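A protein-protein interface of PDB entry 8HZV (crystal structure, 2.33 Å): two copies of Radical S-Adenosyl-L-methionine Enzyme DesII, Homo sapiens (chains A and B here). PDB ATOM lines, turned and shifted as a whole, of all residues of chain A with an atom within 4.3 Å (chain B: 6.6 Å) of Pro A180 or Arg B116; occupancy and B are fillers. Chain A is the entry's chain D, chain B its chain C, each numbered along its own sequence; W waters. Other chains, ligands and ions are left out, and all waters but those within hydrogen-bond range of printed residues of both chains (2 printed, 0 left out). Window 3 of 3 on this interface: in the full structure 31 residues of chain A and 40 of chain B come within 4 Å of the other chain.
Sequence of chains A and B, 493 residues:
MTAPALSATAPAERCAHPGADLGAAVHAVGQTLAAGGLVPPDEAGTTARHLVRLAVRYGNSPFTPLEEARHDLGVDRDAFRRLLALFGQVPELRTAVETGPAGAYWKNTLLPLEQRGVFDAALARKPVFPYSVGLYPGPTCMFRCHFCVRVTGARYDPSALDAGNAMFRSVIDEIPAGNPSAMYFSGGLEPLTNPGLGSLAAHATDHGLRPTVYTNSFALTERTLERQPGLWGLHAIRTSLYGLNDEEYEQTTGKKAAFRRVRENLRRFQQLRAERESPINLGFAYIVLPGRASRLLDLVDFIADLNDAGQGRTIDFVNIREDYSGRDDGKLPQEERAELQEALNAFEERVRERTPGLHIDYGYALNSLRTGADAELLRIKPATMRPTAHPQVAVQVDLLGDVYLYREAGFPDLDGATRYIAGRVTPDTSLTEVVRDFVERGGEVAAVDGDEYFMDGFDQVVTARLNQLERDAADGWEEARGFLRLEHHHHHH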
ATOM      1  N   ARG A 116       2.659  13.538   0.664  1.00  0.00           N
ATOM      2  CA  ARG A 116       3.519  14.651   0.290  1.00  0.00           C
ATOM      3  C   ARG A 116       3.307  15.887   1.154  1.00  0.00           C
ATOM      4  O   ARG A 116       3.967  16.906   0.921  1.00  0.00           O
ATOM      5  CB  ARG A 116       3.281  14.997  -1.184  1.00  0.00           C
ATOM      6  CG  ARG A 116       3.667  13.887  -2.160  1.00  0.00           C
ATOM      7  CD  ARG A 116       3.396  14.306  -3.594  1.00  0.00           C
ATOM      8  NE  ARG A 116       4.555  14.099  -4.459  1.00  0.00           N
ATOM      9  CZ  ARG A 116       5.588  14.936  -4.544  1.00  0.00           C
ATOM     10  NH1 ARG A 116       5.608  16.048  -3.820  1.00  0.00           N
ATOM     11  NH2 ARG A 116       6.599  14.660  -5.359  1.00  0.00           N
ATOM     12  N   GLY A 178      11.826  18.620  -7.383  1.00  0.00           N
ATOM     13  CA  GLY A 178      11.193  17.566  -6.621  1.00  0.00           C
ATOM     14  C   GLY A 178       9.945  16.987  -7.251  1.00  0.00           C
ATOM     15  O   GLY A 178       9.547  15.873  -6.886  1.00  0.00           O
ATOM     16  N   ASN A 179       9.308  17.705  -8.176  1.00  0.00           N
ATOM     17  CA  ASN A 179       8.098  17.223  -8.842  1.00  0.00           C
ATOM     18  C   ASN A 179       8.116  17.699 -10.285  1.00  0.00           C
ATOM     19  O   ASN A 179       7.567  18.759 -10.613  1.00  0.00           O
ATOM     20  CB  ASN A 179       6.834  17.694  -8.118  1.00  0.00           C
ATOM     21  CG  ASN A 179       5.562  17.108  -8.711  1.00  0.00           C
ATOM     22  OD1 ASN A 179       5.607  16.214  -9.556  1.00  0.00           O
ATOM     23  ND2 ASN A 179       4.418  17.615  -8.267  1.00  0.00           N
ATOM     24  N   PRO A 180       8.744  16.936 -11.183  1.00  0.00           N
ATOM     25  CA  PRO A 180       8.816  17.358 -12.593  1.00  0.00           C
ATOM     26  C   PRO A 180       7.462  17.520 -13.275  1.00  0.00           C
ATOM     27  O   PRO A 180       7.423  18.061 -14.388  1.00  0.00           O
ATOM     28  CB  PRO A 180       9.649  16.247 -13.259  1.00  0.00           C
ATOM     29  CG  PRO A 180       9.759  15.147 -12.245  1.00  0.00           C
ATOM     30  CD  PRO A 180       9.599  15.772 -10.903  1.00  0.00           C
ATOM     31  N   SER A 181       6.360  17.092 -12.656  1.00  0.00           N
ATOM     32  CA  SER A 181       5.032  17.296 -13.225  1.00  0.00           C
ATOM     33  C   SER A 181       4.204  18.303 -12.428  1.00  0.00           C
ATOM     34  O   SER A 181       2.971  18.269 -12.484  1.00  0.00           O
ATOM     35  CB  SER A 181       4.288  15.963 -13.337  1.00  0.00           C
ATOM     36  OG  SER A 181       4.235  15.294 -12.092  1.00  0.00           O
ATOM     37  N   ALA A 182       4.858  19.210 -11.696  1.00  0.00           N
ATOM     38  CA  ALA A 182       4.123  20.181 -10.892  1.00  0.00           C
ATOM     39  C   ALA A 182       3.339  21.164 -11.754  1.00  0.00           C
ATOM     40  O   ALA A 182       2.296  21.667 -11.322  1.00  0.00           O
ATOM     41  CB  ALA A 182       5.084  20.938  -9.976  1.00  0.00           C
ATOM     42  N   GLY A 208      14.048  21.522 -16.189  1.00  0.00           N
ATOM     43  CA  GLY A 208      13.966  20.196 -15.616  1.00  0.00           C
ATOM     44  C   GLY A 208      12.566  19.649 -15.460  1.00  0.00           C
ATOM     45  O   GLY A 208      12.397  18.610 -14.813  1.00  0.00           O
ATOM     46  N   LEU A 209      11.562  20.311 -16.030  1.00  0.00           N
ATOM     47  CA  LEU A 209      10.172  19.903 -15.886  1.00  0.00           C
ATOM     48  C   LEU A 209       9.742  19.005 -17.041  1.00  0.00           C
ATOM     49  O   LEU A 209      10.338  19.005 -18.121  1.00  0.00           O
ATOM     50  CB  LEU A 209       9.258  21.126 -15.813  1.00  0.00           C
ATOM     51  CG  LEU A 209       9.539  22.070 -14.648  1.00  0.00           C
ATOM     52  CD1 LEU A 209       8.817  23.401 -14.837  1.00  0.00           C
ATOM     53  CD2 LEU A 209       9.151  21.413 -13.326  1.00  0.00           C
ATOM     54  N   ARG A 210       8.680  18.237 -16.798  1.00  0.00           N
ATOM     55  CA  ARG A 210       8.095  17.336 -17.792  1.00  0.00           C
ATOM     56  C   ARG A 210       6.599  17.612 -17.840  1.00  0.00           C
ATOM     57  O   ARG A 210       5.797  16.872 -17.252  1.00  0.00           O
ATOM     58  CB  ARG A 210       8.401  15.874 -17.462  1.00  0.00           C
ATOM     59  CG  ARG A 210       9.895  15.563 -17.442  1.00  0.00           C
ATOM     60  CD  ARG A 210      10.186  14.114 -17.074  1.00  0.00           C
ATOM     61  NE  ARG A 210      11.620  13.887 -16.900  1.00  0.00           N
ATOM     62  CZ  ARG A 210      12.421  13.389 -17.840  1.00  0.00           C
ATOM     63  NH1 ARG A 210      13.713  13.224 -17.592  1.00  0.00           N
ATOM     64  NH2 ARG A 210      11.930  13.058 -19.028  1.00  0.00           N
ATOM     65  N   LEU B 111      12.481   3.465  -8.829  1.00  0.00           N
ATOM     66  CA  LEU B 111      11.372   4.128  -9.509  1.00  0.00           C
ATOM     67  C   LEU B 111      10.888   5.384  -8.783  1.00  0.00           C
ATOM     68  O   LEU B 111      10.603   6.387  -9.449  1.00  0.00           O
ATOM     69  CB  LEU B 111      10.216   3.141  -9.720  1.00  0.00           C
ATOM     70  CG  LEU B 111      10.547   1.989 -10.682  1.00  0.00           C
ATOM     71  CD1 LEU B 111       9.338   1.095 -10.932  1.00  0.00           C
ATOM     72  CD2 LEU B 111      11.100   2.523 -12.000  1.00  0.00           C
ATOM     73  N   PRO B 112      10.770   5.393  -7.445  1.00  0.00           N
ATOM     74  CA  PRO B 112      10.366   6.647  -6.780  1.00  0.00           C
ATOM     75  C   PRO B 112      11.336   7.797  -7.000  1.00  0.00           C
ATOM     76  O   PRO B 112      10.906   8.954  -7.114  1.00  0.00           O
ATOM     77  CB  PRO B 112      10.292   6.249  -5.300  1.00  0.00           C
ATOM     78  CG  PRO B 112      10.030   4.798  -5.318  1.00  0.00           C
ATOM     79  CD  PRO B 112      10.801   4.270  -6.488  1.00  0.00           C
ATOM     80  N   LEU B 113      12.638   7.517  -7.058  1.00  0.00           N
ATOM     81  CA  LEU B 113      13.607   8.596  -7.225  1.00  0.00           C
ATOM     82  C   LEU B 113      13.693   9.067  -8.673  1.00  0.00           C
ATOM     83  O   LEU B 113      13.945  10.250  -8.919  1.00  0.00           O
ATOM     84  CB  LEU B 113      14.979   8.154  -6.715  1.00  0.00           C
ATOM     85  CG  LEU B 113      15.316   8.543  -5.269  1.00  0.00           C
ATOM     86  CD1 LEU B 113      14.318   7.948  -4.284  1.00  0.00           C
ATOM     87  CD2 LEU B 113      16.732   8.119  -4.912  1.00  0.00           C
ATOM     88  N   GLU B 114      13.489   8.170  -9.640  1.00  0.00           N
ATOM     89  CA  GLU B 114      13.360   8.617 -11.022  1.00  0.00           C
ATOM     90  C   GLU B 114      12.129   9.500 -11.188  1.00  0.00           C
ATOM     91  O   GLU B 114      12.156  10.485 -11.936  1.00  0.00           O
ATOM     92  CB  GLU B 114      13.292   7.414 -11.963  1.00  0.00           C
ATOM     93  CG  GLU B 114      14.554   6.561 -11.984  1.00  0.00           C
ATOM     94  CD  GLU B 114      15.606   7.071 -12.958  1.00  0.00           C
ATOM     95  OE1 GLU B 114      15.467   8.207 -13.456  1.00  0.00           O
ATOM     96  OE2 GLU B 114      16.574   6.327 -13.225  1.00  0.00           O
ATOM     97  N   GLN B 115      11.046   9.168 -10.479  1.00  0.00           N
ATOM     98  CA  GLN B 115       9.811   9.941 -10.559  1.00  0.00           C
ATOM     99  C   GLN B 115      10.026  11.375 -10.095  1.00  0.00           C
ATOM    100  O   GLN B 115       9.477  12.318 -10.681  1.00  0.00           O
ATOM    101  CB  GLN B 115       8.721   9.264  -9.726  1.00  0.00           C
ATOM    102  CG  GLN B 115       7.349   9.224 -10.381  1.00  0.00           C
ATOM    103  CD  GLN B 115       7.248   8.169 -11.469  1.00  0.00           C
ATOM    104  OE1 GLN B 115       8.156   7.357 -11.651  1.00  0.00           O
ATOM    105  NE2 GLN B 115       6.137   8.176 -12.200  1.00  0.00           N
ATOM    106  N   ARG B 116      10.803  11.561  -9.032  1.00  0.00           N
ATOM    107  CA  ARG B 116      11.094  12.893  -8.524  1.00  0.00           C
ATOM    108  C   ARG B 116      12.189  13.599  -9.315  1.00  0.00           C
ATOM    109  O   ARG B 116      12.547  14.731  -8.974  1.00  0.00           O
ATOM    110  CB  ARG B 116      11.493  12.813  -7.047  1.00  0.00           C
ATOM    111  CG  ARG B 116      10.366  12.381  -6.114  1.00  0.00           C
ATOM    112  CD  ARG B 116      10.861  12.265  -4.678  1.00  0.00           C
ATOM    113  NE  ARG B 116       9.773  12.088  -3.719  1.00  0.00           N
ATOM    114  CZ  ARG B 116       9.131  13.090  -3.123  1.00  0.00           C
ATOM    115  NH1 ARG B 116       9.463  14.347  -3.391  1.00  0.00           N
ATOM    116  NH2 ARG B 116       8.153  12.836  -2.261  1.00  0.00           N
ATOM    117  N   GLY B 117      12.727  12.970 -10.358  1.00  0.00           N
ATOM    118  CA  GLY B 117      13.822  13.573 -11.091  1.00  0.00           C
ATOM    119  C   GLY B 117      15.114  13.667 -10.315  1.00  0.00           C
ATOM    120  O   GLY B 117      15.994  14.448 -10.687  1.00  0.00           O
ATOM    121  N   VAL B 118      15.255  12.888  -9.243  1.00  0.00           N
ATOM    122  CA  VAL B 118      16.461  12.951  -8.425  1.00  0.00           C
ATOM    123  C   VAL B 118      17.653  12.377  -9.183  1.00  0.00           C
ATOM    124  O   VAL B 118      18.733  12.979  -9.220  1.00  0.00           O
ATOM    125  CB  VAL B 118      16.235  12.223  -7.089  1.00  0.00           C
ATOM    126  CG1 VAL B 118      17.514  12.208  -6.270  1.00  0.00           C
ATOM    127  CG2 VAL B 118      15.112  12.889  -6.318  1.00  0.00           C
ATOM    128  N   PHE B 119      17.473  11.208  -9.802  1.00  0.00           N
ATOM    129  CA  PHE B 119      18.567  10.596 -10.550  1.00  0.00           C
ATOM    130  C   PHE B 119      18.980  11.460 -11.737  1.00  0.00           C
ATOM    131  O   PHE B 119      20.175  11.585 -12.035  1.00  0.00           O
ATOM    132  CB  PHE B 119      18.169   9.194 -11.014  1.00  0.00           C
ATOM    133  CG  PHE B 119      18.327   8.142  -9.955  1.00  0.00           C
ATOM    134  CD1 PHE B 119      19.561   7.911  -9.372  1.00  0.00           C
ATOM    135  CD2 PHE B 119      17.239   7.387  -9.536  1.00  0.00           C
ATOM    136  CE1 PHE B 119      19.713   6.943  -8.389  1.00  0.00           C
ATOM    137  CE2 PHE B 119      17.381   6.421  -8.556  1.00  0.00           C
ATOM    138  CZ  PHE B 119      18.620   6.198  -7.979  1.00  0.00           C
ATOM    139  N   TYR B 131      18.223  15.529  -2.165  1.00  0.00           N
ATOM    140  CA  TYR B 131      16.928  14.897  -1.942  1.00  0.00           C
ATOM    141  C   TYR B 131      16.790  14.394  -0.510  1.00  0.00           C
ATOM    142  O   TYR B 131      15.689  14.413   0.049  1.00  0.00           O
ATOM    143  CB  TYR B 131      16.723  13.754  -2.940  1.00  0.00           C
ATOM    144  CG  TYR B 131      15.774  12.671  -2.467  1.00  0.00           C
ATOM    145  CD1 TYR B 131      14.396  12.854  -2.516  1.00  0.00           C
ATOM    146  CD2 TYR B 131      16.256  11.462  -1.978  1.00  0.00           C
ATOM    147  CE1 TYR B 131      13.526  11.862  -2.085  1.00  0.00           C
ATOM    148  CE2 TYR B 131      15.396  10.467  -1.546  1.00  0.00           C
ATOM    149  CZ  TYR B 131      14.033  10.672  -1.600  1.00  0.00           C
ATOM    150  OH  TYR B 131      13.180   9.681  -1.166  1.00  0.00           O
ATOM    151  N   GLY B 178       7.540  20.179   0.084  1.00  0.00           N
ATOM    152  CA  GLY B 178       7.197  19.154  -0.878  1.00  0.00           C
ATOM    153  C   GLY B 178       7.569  17.751  -0.449  1.00  0.00           C
ATOM    154  O   GLY B 178       7.052  16.781  -1.023  1.00  0.00           O
ATOM    155  N   ASN B 179       8.448  17.614   0.542  1.00  0.00           N
ATOM    156  CA  ASN B 179       8.855  16.307   1.054  1.00  0.00           C
ATOM    157  C   ASN B 179       9.048  16.430   2.556  1.00  0.00           C
ATOM    158  O   ASN B 179      10.160  16.682   3.037  1.00  0.00           O
ATOM    159  CB  ASN B 179      10.131  15.811   0.374  1.00  0.00           C
ATOM    160  CG  ASN B 179      10.487  14.393   0.768  1.00  0.00           C
ATOM    161  OD1 ASN B 179       9.742  13.732   1.496  1.00  0.00           O
ATOM    162  ND2 ASN B 179      11.630  13.914   0.287  1.00  0.00           N
ATOM    163  N   PRO B 180       7.978  16.248   3.336  1.00  0.00           N
ATOM    164  CA  PRO B 180       8.081  16.456   4.792  1.00  0.00           C
ATOM    165  C   PRO B 180       9.034  15.498   5.499  1.00  0.00           C
ATOM    166  O   PRO B 180       9.322  15.717   6.681  1.00  0.00           O
ATOM    167  CB  PRO B 180       6.635  16.271   5.280  1.00  0.00           C
ATOM    168  CG  PRO B 180       5.946  15.510   4.186  1.00  0.00           C
ATOM    169  CD  PRO B 180       6.603  15.934   2.911  1.00  0.00           C
HETATM  170  O   HOH W   1      13.508  17.372  -9.435  1.00  0.00           O
HETATM  171  O   HOH W   2       4.550  19.560   1.725  1.00  0.00           O
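Arg A116 touches Pro B180. Gly A178 touches Arg B116. Pro A180 touches Gln B115 (CG to O, 3.2 Å). Pro A180 touches Arg B116.
Pro A180 touches two residues of chain B. Arg B116 touches just these residues of chain A: Arg A116 (3.5 Å), Gly A178 (3.6 Å) and Pro A180 (3.7 Å). Of the printed residues of chain B, Gly A178 touches Arg B116. Printed residues of chain A within 4 Å of Gln B115: Pro A180 (3.2 Å). Printed residues of chain A within 4 Å of Pro B180: Arg A116. Of the printed residues of chain A, Gly B178 touches Arg A116 (3.2 Å). Gly B117 touches none of the printed residues of chain A. The nearest printed residue of chain A that does not touch Arg B116 is Asn A179 (4.5 Å). The nearest printed residue of chain A that does not touch Pro B180 is Gly A178 (10.2 Å).
The backbone carbonyl oxygen (O) of Leu B111 sits close to the side-chain amide oxygen (OE1) of Gln B115 (3.4 Å). The backbone carbonyl oxygen (O) of Pro A180 lies within hydrogen-bond range of the backbone NH (N) of Arg A210, at 2.7 Å.
Water W2 lies within hydrogen-bond range of O of Arg A116 (2.8 Å) and N of Gly B178 (3.5 Å). Water W1 bridges the backbone carbonyl oxygen of Arg B116 and the backbone NH of Gly A178.
The backbone carbonyl oxygen (O) of Gly B178 is in hydrogen-bond range of the guanidinium group (NH1) of Arg A116 (3.2 Å). NH2 of Arg A116 sits close to NH1 of Arg B116, at 3.5 Å.
Printed residues of chain A that touch a printed residue of chain B: Arg A116, Gly A178 and Pro A180. Of the 13 printed residues of chain B, 4 touch a printed residue of chain A. Among the printed residues, 6 pairs touch across the chains. Among the printed residues, no Asp or Glu carboxylate lies within 4 Å of a Lys or Arg side-chain nitrogen of the other chain.
Arg B116 touches its own counterpart, Arg A116. Arg A116 touches Gly B178, and with the chains exchanged Gly A178 touches Arg B116. Arg A116 touches Pro B180, and with the chains exchanged Pro A180 touches Arg B116. Of the 6 pairs that touch across the chains among the printed residues, 5 have their exchanged pair printed and touching as well.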
